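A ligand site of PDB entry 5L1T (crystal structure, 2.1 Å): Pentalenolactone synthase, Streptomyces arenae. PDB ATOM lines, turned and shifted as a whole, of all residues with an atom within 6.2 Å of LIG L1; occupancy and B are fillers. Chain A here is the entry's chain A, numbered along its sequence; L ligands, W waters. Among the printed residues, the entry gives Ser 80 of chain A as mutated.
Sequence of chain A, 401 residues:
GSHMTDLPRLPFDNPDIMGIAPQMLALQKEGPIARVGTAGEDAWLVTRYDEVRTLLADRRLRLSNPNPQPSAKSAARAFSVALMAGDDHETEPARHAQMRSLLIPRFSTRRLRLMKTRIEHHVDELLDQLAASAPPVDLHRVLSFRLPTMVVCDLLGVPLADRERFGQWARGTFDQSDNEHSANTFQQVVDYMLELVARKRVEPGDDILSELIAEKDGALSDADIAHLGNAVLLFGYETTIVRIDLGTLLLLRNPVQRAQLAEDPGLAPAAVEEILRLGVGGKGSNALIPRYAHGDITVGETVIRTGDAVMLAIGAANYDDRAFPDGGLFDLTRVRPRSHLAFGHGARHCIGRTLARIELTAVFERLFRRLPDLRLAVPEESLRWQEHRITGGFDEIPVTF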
ATOM      1  N   ARG A  77      21.477  11.238 -19.988  1.00  0.00           N
ATOM      2  CA  ARG A  77      22.644  11.768 -19.290  1.00  0.00           C
ATOM      3  C   ARG A  77      22.500  13.254 -19.005  1.00  0.00           C
ATOM      4  O   ARG A  77      22.961  13.747 -17.961  1.00  0.00           O
ATOM      5  CB  ARG A  77      23.919  11.513 -20.099  1.00  0.00           C
ATOM      6  CG  ARG A  77      24.481  10.114 -19.970  1.00  0.00           C
ATOM      7  CD  ARG A  77      25.001   9.863 -18.551  1.00  0.00           C
ATOM      8  NE  ARG A  77      25.450   8.487 -18.384  1.00  0.00           N
ATOM      9  CZ  ARG A  77      25.990   7.998 -17.268  1.00  0.00           C
ATOM     10  NH1 ARG A  77      26.150   8.782 -16.208  1.00  0.00           N
ATOM     11  NH2 ARG A  77      26.365   6.732 -17.222  1.00  0.00           N
ATOM     12  N   SER A  80      20.374  13.544 -15.850  1.00  0.00           N
ATOM     13  CA  SER A  80      21.062  13.164 -14.623  1.00  0.00           C
ATOM     14  C   SER A  80      22.019  14.261 -14.181  1.00  0.00           C
ATOM     15  O   SER A  80      22.153  14.527 -12.980  1.00  0.00           O
ATOM     16  CB  SER A  80      21.813  11.844 -14.831  1.00  0.00           C
ATOM     17  OG  SER A  80      22.748  11.961 -15.890  1.00  0.00           O
ATOM     18  N   MET A  84      21.669  16.987 -10.758  1.00  0.00           N
ATOM     19  CA  MET A  84      22.798  17.159  -9.851  1.00  0.00           C
ATOM     20  C   MET A  84      23.416  18.557  -9.944  1.00  0.00           C
ATOM     21  O   MET A  84      24.561  18.752  -9.499  1.00  0.00           O
ATOM     22  CB  MET A  84      23.856  16.089 -10.136  1.00  0.00           C
ATOM     23  CG  MET A  84      23.375  14.661  -9.828  1.00  0.00           C
ATOM     24  SD  MET A  84      24.440  13.331 -10.454  1.00  0.00           S
ATOM     25  CE  MET A  84      25.818  13.408  -9.315  1.00  0.00           C
ATOM     26  N   PHE A 174      16.149   7.531 -17.553  1.00  0.00           N
ATOM     27  CA  PHE A 174      17.551   7.177 -17.757  1.00  0.00           C
ATOM     28  C   PHE A 174      17.755   6.186 -18.900  1.00  0.00           C
ATOM     29  O   PHE A 174      18.797   5.516 -18.959  1.00  0.00           O
ATOM     30  CB  PHE A 174      18.153   6.632 -16.458  1.00  0.00           C
ATOM     31  CG  PHE A 174      18.128   7.629 -15.322  1.00  0.00           C
ATOM     32  CD1 PHE A 174      18.262   8.981 -15.576  1.00  0.00           C
ATOM     33  CD2 PHE A 174      17.953   7.204 -14.013  1.00  0.00           C
ATOM     34  CE1 PHE A 174      18.241   9.913 -14.544  1.00  0.00           C
ATOM     35  CE2 PHE A 174      17.913   8.126 -12.971  1.00  0.00           C
ATOM     36  CZ  PHE A 174      18.063   9.480 -13.240  1.00  0.00           C
ATOM     37  N   LEU A 234      14.131  10.218  -8.448  1.00  0.00           N
ATOM     38  CA  LEU A 234      14.818   9.505  -9.518  1.00  0.00           C
ATOM     39  C   LEU A 234      16.121   8.856  -9.063  1.00  0.00           C
ATOM     40  O   LEU A 234      16.543   7.861  -9.662  1.00  0.00           O
ATOM     41  CB  LEU A 234      15.067  10.444 -10.714  1.00  0.00           C
ATOM     42  CG  LEU A 234      13.795  10.859 -11.465  1.00  0.00           C
ATOM     43  CD1 LEU A 234      13.975  12.217 -12.150  1.00  0.00           C
ATOM     44  CD2 LEU A 234      13.338   9.769 -12.464  1.00  0.00           C
ATOM     45  N   PHE A 235      16.772   9.379  -8.013  1.00  0.00           N
ATOM     46  CA  PHE A 235      17.947   8.718  -7.447  1.00  0.00           C
ATOM     47  C   PHE A 235      17.604   7.819  -6.256  1.00  0.00           C
ATOM     48  O   PHE A 235      18.437   7.020  -5.831  1.00  0.00           O
ATOM     49  CB  PHE A 235      18.982   9.757  -6.979  1.00  0.00           C
ATOM     50  CG  PHE A 235      19.500  10.656  -8.077  1.00  0.00           C
ATOM     51  CD1 PHE A 235      19.341  10.326  -9.407  1.00  0.00           C
ATOM     52  CD2 PHE A 235      20.118  11.861  -7.764  1.00  0.00           C
ATOM     53  CE1 PHE A 235      19.822  11.155 -10.421  1.00  0.00           C
ATOM     54  CE2 PHE A 235      20.601  12.710  -8.792  1.00  0.00           C
ATOM     55  CZ  PHE A 235      20.446  12.348 -10.110  1.00  0.00           C
ATOM     56  N   THR A 239      18.499   2.507  -7.838  1.00  0.00           N
ATOM     57  CA  THR A 239      19.788   1.876  -7.558  1.00  0.00           C
ATOM     58  C   THR A 239      19.700   0.962  -6.347  1.00  0.00           C
ATOM     59  O   THR A 239      20.444  -0.035  -6.261  1.00  0.00           O
ATOM     60  CB  THR A 239      20.894   2.922  -7.346  1.00  0.00           C
ATOM     61  OG1 THR A 239      20.550   3.797  -6.265  1.00  0.00           O
ATOM     62  CG2 THR A 239      21.133   3.767  -8.606  1.00  0.00           C
ATOM     63  N   ARG A 243      20.667  -3.113  -6.039  1.00  0.00           N
ATOM     64  CA  ARG A 243      21.557  -3.723  -5.038  1.00  0.00           C
ATOM     65  C   ARG A 243      20.878  -4.879  -4.299  1.00  0.00           C
ATOM     66  O   ARG A 243      21.566  -5.827  -3.894  1.00  0.00           O
ATOM     67  CB  ARG A 243      22.060  -2.678  -4.035  1.00  0.00           C
ATOM     68  CG  ARG A 243      22.857  -1.567  -4.736  1.00  0.00           C
ATOM     69  CD  ARG A 243      23.816  -2.173  -5.778  1.00  0.00           C
ATOM     70  NE  ARG A 243      24.728  -1.261  -6.442  1.00  0.00           N
ATOM     71  CZ  ARG A 243      24.380  -0.433  -7.411  1.00  0.00           C
ATOM     72  NH1 ARG A 243      23.119  -0.355  -7.829  1.00  0.00           N
ATOM     73  NH2 ARG A 243      25.295   0.332  -7.989  1.00  0.00           N
ATOM     74  N   SER A 285      28.811  -0.458 -16.751  1.00  0.00           N
ATOM     75  CA  SER A 285      28.952   0.946 -17.145  1.00  0.00           C
ATOM     76  C   SER A 285      28.436   1.908 -16.077  1.00  0.00           C
ATOM     77  O   SER A 285      28.826   3.079 -16.082  1.00  0.00           O
ATOM     78  CB  SER A 285      28.204   1.193 -18.462  1.00  0.00           C
ATOM     79  OG  SER A 285      28.736   0.369 -19.483  1.00  0.00           O
ATOM     80  N   ASN A 286      27.552   1.439 -15.185  1.00  0.00           N
ATOM     81  CA  ASN A 286      27.075   2.273 -14.089  1.00  0.00           C
ATOM     82  C   ASN A 286      28.046   2.277 -12.923  1.00  0.00           C
ATOM     83  O   ASN A 286      27.867   3.069 -11.983  1.00  0.00           O
ATOM     84  CB  ASN A 286      25.690   1.792 -13.621  1.00  0.00           C
ATOM     85  CG  ASN A 286      25.716   0.404 -13.027  1.00  0.00           C
ATOM     86  OD1 ASN A 286      26.262  -0.550 -13.612  1.00  0.00           O
ATOM     87  ND2 ASN A 286      25.124   0.267 -11.850  1.00  0.00           N
ATOM     88  N   ALA A 287      29.082   1.427 -12.937  1.00  0.00           N
ATOM     89  CA  ALA A 287      30.129   1.477 -11.928  1.00  0.00           C
ATOM     90  C   ALA A 287      31.282   2.393 -12.338  1.00  0.00           C
ATOM     91  O   ALA A 287      32.430   2.158 -11.950  1.00  0.00           O
ATOM     92  CB  ALA A 287      30.642   0.077 -11.612  1.00  0.00           C
ATOM     93  N   LEU A 288      30.990   3.413 -13.127  1.00  0.00           N
ATOM     94  CA  LEU A 288      31.947   4.443 -13.492  1.00  0.00           C
ATOM     95  C   LEU A 288      31.357   5.798 -13.114  1.00  0.00           C
ATOM     96  O   LEU A 288      30.203   6.074 -13.442  1.00  0.00           O
ATOM     97  CB  LEU A 288      32.225   4.404 -14.999  1.00  0.00           C
ATOM     98  CG  LEU A 288      32.645   3.111 -15.712  1.00  0.00           C
ATOM     99  CD1 LEU A 288      32.775   3.388 -17.203  1.00  0.00           C
ATOM    100  CD2 LEU A 288      33.965   2.606 -15.160  1.00  0.00           C
ATOM    101  N   ILE A 289      32.137   6.609 -12.408  1.00  0.00           N
ATOM    102  CA  ILE A 289      31.741   7.963 -12.057  1.00  0.00           C
ATOM    103  C   ILE A 289      32.367   8.908 -13.075  1.00  0.00           C
ATOM    104  O   ILE A 289      33.604   8.947 -13.172  1.00  0.00           O
ATOM    105  CB  ILE A 289      32.155   8.341 -10.624  1.00  0.00           C
ATOM    106  CG1 ILE A 289      31.327   7.539  -9.611  1.00  0.00           C
ATOM    107  CG2 ILE A 289      31.991   9.835 -10.426  1.00  0.00           C
ATOM    108  CD1 ILE A 289      31.598   7.957  -8.171  1.00  0.00           C
ATOM    109  N   PRO A 290      31.580   9.639 -13.865  1.00  0.00           N
ATOM    110  CA  PRO A 290      32.157  10.500 -14.915  1.00  0.00           C
ATOM    111  C   PRO A 290      32.492  11.889 -14.385  1.00  0.00           C
ATOM    112  O   PRO A 290      31.779  12.458 -13.557  1.00  0.00           O
ATOM    113  CB  PRO A 290      31.021  10.579 -15.940  1.00  0.00           C
ATOM    114  CG  PRO A 290      29.773  10.523 -15.073  1.00  0.00           C
ATOM    115  CD  PRO A 290      30.109   9.678 -13.871  1.00  0.00           C
ATOM    116  N   ILE A 314      34.785   3.064  -9.973  1.00  0.00           N
ATOM    117  CA  ILE A 314      34.569   2.668  -8.579  1.00  0.00           C
ATOM    118  C   ILE A 314      34.362   1.157  -8.466  1.00  0.00           C
ATOM    119  O   ILE A 314      34.760   0.545  -7.462  1.00  0.00           O
ATOM    120  CB  ILE A 314      33.400   3.477  -7.966  1.00  0.00           C
ATOM    121  CG1 ILE A 314      32.096   3.256  -8.751  1.00  0.00           C
ATOM    122  CG2 ILE A 314      33.758   4.981  -7.871  1.00  0.00           C
ATOM    123  CD1 ILE A 314      30.885   3.997  -8.160  1.00  0.00           C
ATOM    124  N   ALA A 342      31.454   2.362  -3.498  1.00  0.00           N
ATOM    125  CA  ALA A 342      30.181   2.193  -4.202  1.00  0.00           C
ATOM    126  C   ALA A 342      29.222   3.372  -4.028  1.00  0.00           C
ATOM    127  O   ALA A 342      28.331   3.546  -4.855  1.00  0.00           O
ATOM    128  CB  ALA A 342      29.471   0.907  -3.748  1.00  0.00           C
ATOM    129  N   ILE A 390      21.104   4.068 -17.616  1.00  0.00           N
ATOM    130  CA  ILE A 390      22.213   4.573 -16.791  1.00  0.00           C
ATOM    131  C   ILE A 390      22.390   3.710 -15.554  1.00  0.00           C
ATOM    132  O   ILE A 390      23.516   3.360 -15.184  1.00  0.00           O
ATOM    133  CB  ILE A 390      21.981   6.047 -16.422  1.00  0.00           C
ATOM    134  CG1 ILE A 390      22.119   6.955 -17.659  1.00  0.00           C
ATOM    135  CG2 ILE A 390      22.961   6.465 -15.329  1.00  0.00           C
ATOM    136  CD1 ILE A 390      21.631   8.363 -17.424  1.00  0.00           C
ATOM    137  N   THR A 391      21.277   3.312 -14.929  1.00  0.00           N
ATOM    138  CA  THR A 391      21.294   2.505 -13.721  1.00  0.00           C
ATOM    139  C   THR A 391      21.289   0.991 -13.982  1.00  0.00           C
ATOM    140  O   THR A 391      21.210   0.213 -13.018  1.00  0.00           O
ATOM    141  CB  THR A 391      20.100   2.897 -12.847  1.00  0.00           C
ATOM    142  OG1 THR A 391      18.947   3.018 -13.676  1.00  0.00           O
ATOM    143  CG2 THR A 391      20.366   4.237 -12.203  1.00  0.00           C
ATOM    144  N   GLY A 392      21.385   0.543 -15.238  1.00  0.00           N
ATOM    145  CA  GLY A 392      21.549  -0.882 -15.515  1.00  0.00           C
ATOM    146  C   GLY A 392      20.405  -1.703 -14.936  1.00  0.00           C
ATOM    147  O   GLY A 392      19.233  -1.357 -15.095  1.00  0.00           O
HETATM  148  C1  LIG L   1      24.314   7.673  -8.572  1.00  0.00           C
HETATM  149  C2  LIG L   1      23.477   8.361  -9.658  1.00  0.00           C
HETATM  150  C3  LIG L   1      23.206   9.803  -9.250  1.00  0.00           C
HETATM  151  C4  LIG L   1      22.114   7.660  -9.871  1.00  0.00           C
HETATM  152  C5  LIG L   1      25.128   5.328  -9.138  1.00  0.00           C
HETATM  153  C6  LIG L   1      25.118   5.237 -12.549  1.00  0.00           C
HETATM  154  C7  LIG L   1      27.793   6.411 -10.927  1.00  0.00           C
HETATM  155  C8  LIG L   1      24.429   8.328 -10.872  1.00  0.00           C
HETATM  156  C9  LIG L   1      24.271   3.451 -10.377  1.00  0.00           C
HETATM  157  C10 LIG L   1      26.437   7.233 -12.881  1.00  0.00           C
HETATM  158  C11 LIG L   1      24.541   4.788 -10.246  1.00  0.00           C
HETATM  159  C12 LIG L   1      25.357   6.737  -9.280  1.00  0.00           C
HETATM  160  C13 LIG L   1      24.397   5.773 -11.270  1.00  0.00           C
HETATM  161  C14 LIG L   1      26.578   7.109 -11.486  1.00  0.00           C
HETATM  162  C15 LIG L   1      25.192   6.980 -10.781  1.00  0.00           C
HETATM  163  O1  LIG L   1      24.571   2.631  -9.474  1.00  0.00           O
HETATM  164  O2  LIG L   1      26.982   8.161 -13.489  1.00  0.00           O
HETATM  165  O3  LIG L   1      23.664   2.974 -11.366  1.00  0.00           O
HETATM  166  O4  LIG L   1      25.608   6.302 -13.469  1.00  0.00           O
HETATM  167  O5  LIG L   1      27.603   7.863 -10.851  1.00  0.00           O
HETATM  168  C1  LG2 L   2      24.991  10.354  -5.422  1.00  0.00           C
HETATM  169  C2  LG2 L   2      25.269   5.491  -5.407  1.00  0.00           C
HETATM  170  C3  LG2 L   2      21.033   5.245  -3.054  1.00  0.00           C
HETATM  171  C4  LG2 L   2      20.574  10.082  -3.326  1.00  0.00           C
HETATM  172  C5  LG2 L   2      25.487   9.077  -5.592  1.00  0.00           C
HETATM  173  C6  LG2 L   2      26.793   8.684  -6.135  1.00  0.00           C
HETATM  174  C7  LG2 L   2      26.841   7.335  -6.122  1.00  0.00           C
HETATM  175  C8  LG2 L   2      25.595   6.829  -5.576  1.00  0.00           C
HETATM  176  C9  LG2 L   2      28.014   6.444  -6.612  1.00  0.00           C
HETATM  177  C10 LG2 L   2      27.927   9.639  -6.621  1.00  0.00           C
HETATM  178  C11 LG2 L   2      27.702  10.204  -8.029  1.00  0.00           C
HETATM  179  C12 LG2 L   2      28.880  11.072  -8.457  1.00  0.00           C
HETATM  180  O1  LG2 L   2      29.882  11.180  -7.692  1.00  0.00           O
HETATM  181  O2  LG2 L   2      28.835  11.658  -9.574  1.00  0.00           O
HETATM  182  C13 LG2 L   2      24.154   4.972  -4.758  1.00  0.00           C
HETATM  183  C14 LG2 L   2      23.889   3.567  -4.469  1.00  0.00           C
HETATM  184  C15 LG2 L   2      22.708   3.504  -3.830  1.00  0.00           C
HETATM  185  C16 LG2 L   2      22.204   4.866  -3.678  1.00  0.00           C
HETATM  186  C17 LG2 L   2      24.819   2.396  -4.875  1.00  0.00           C
HETATM  187  C18 LG2 L   2      21.950   2.265  -3.276  1.00  0.00           C
HETATM  188  C19 LG2 L   2      22.582   1.158  -2.852  1.00  0.00           C
HETATM  189  C20 LG2 L   2      20.548   6.537  -2.896  1.00  0.00           C
HETATM  190  C21 LG2 L   2      19.337   6.878  -2.199  1.00  0.00           C
HETATM  191  C22 LG2 L   2      19.185   8.224  -2.263  1.00  0.00           C
HETATM  192  C23 LG2 L   2      20.317   8.763  -3.024  1.00  0.00           C
HETATM  193  C24 LG2 L   2      18.426   5.808  -1.513  1.00  0.00           C
HETATM  194  C25 LG2 L   2      18.059   9.112  -1.693  1.00  0.00           C
HETATM  195  C26 LG2 L   2      16.881   8.655  -1.260  1.00  0.00           C
HETATM  196  C27 LG2 L   2      21.699  10.580  -3.966  1.00  0.00           C
HETATM  197  C28 LG2 L   2      21.930  11.942  -4.392  1.00  0.00           C
HETATM  198  C29 LG2 L   2      23.138  12.014  -4.980  1.00  0.00           C
HETATM  199  C30 LG2 L   2      23.728  10.701  -4.958  1.00  0.00           C
HETATM  200  C31 LG2 L   2      20.924  13.100  -4.213  1.00  0.00           C
HETATM  201  C32 LG2 L   2      23.796  13.282  -5.582  1.00  0.00           C
HETATM  202  C33 LG2 L   2      24.823  13.836  -4.613  1.00  0.00           C
HETATM  203  C34 LG2 L   2      25.569  15.026  -5.180  1.00  0.00           C
HETATM  204  O3  LG2 L   2      26.141  15.802  -4.374  1.00  0.00           O
HETATM  205  O4  LG2 L   2      25.602  15.190  -6.443  1.00  0.00           O
HETATM  206  N1  LG2 L   2      24.805   7.917  -5.253  1.00  0.00           N
HETATM  207  N2  LG2 L   2      23.107   5.719  -4.252  1.00  0.00           N
HETATM  208  N3  LG2 L   2      21.110   7.700  -3.395  1.00  0.00           N
HETATM  209  N4  LG2 L   2      22.822   9.853  -4.324  1.00  0.00           N
HETATM  210 FE1  LG2 L   2      23.058   7.811  -4.054  1.00  0.00          FE
HETATM  211  O   HOH W   1      27.372   3.061  -9.207  1.00  0.00           O
HETATM  212  O   HOH W   2      22.227   0.760 -10.413  1.00  0.00           O
HETATM  213  O   HOH W   3      28.399   5.759 -15.499  1.00  0.00           O
HETATM  214  O   HOH W   4      27.602  10.754 -11.868  1.00  0.00           O
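Residues that only touch LIG L1: Met 84 (3.9 Å), Phe 235 (3.8 Å), Thr 239 (3.6 Å), Leu 288 (3.5 Å), Ile 289 (3.9 Å), Pro 290 (3.5 Å), Ile 390 (3.2 Å) and Thr 391 (3.4 Å). Hydrophobic or aromatic side chains within 4 Å of LIG L1: Met 84, Phe 235, Ile 289, Pro 290 and Ile 390. Of the 19 residues printed, 11 come within 4 Å of LIG L1.
NH1 of Arg 243 is in hydrogen-bond range of O of Thr 239, at 3.1 Å. The side-chain hydroxyl of Ser 80 is in hydrogen-bond range of the backbone carbonyl oxygen of Arg 77. The backbone NH (N) of Ile 390 sits at hydrogen-bond distance from the backbone carbonyl oxygen (O) of Phe 174, at 3.0 Å.
Water W2 lies within hydrogen-bond range of O3 of LIG L1 (2.8 Å), O of Thr 391 (2.8 Å), NH1 of Arg 243 (3.0 Å) and ND2 of Asn 286 (3.3 Å). Water W1 bridges the backbone carbonyl oxygen (O) of Asn 286 and an oxygen (O1) of LIG L1. Water W4 bridges an oxygen (O2) of LG2 L2 and an oxygen (O5) of LIG L1.
The guanidinium group of Arg 243 is in salt-bridge range of an oxygen (O1) of LIG L1. The guanidinium group of Arg 77 sits at hydrogen-bond distance from an oxygen (O2) of LIG L1, 2.9 Å away. An oxygen (O3) of LIG L1 lies within hydrogen-bond range of the side-chain amide nitrogen (ND2) of Asn 286, 3.1 Å away.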
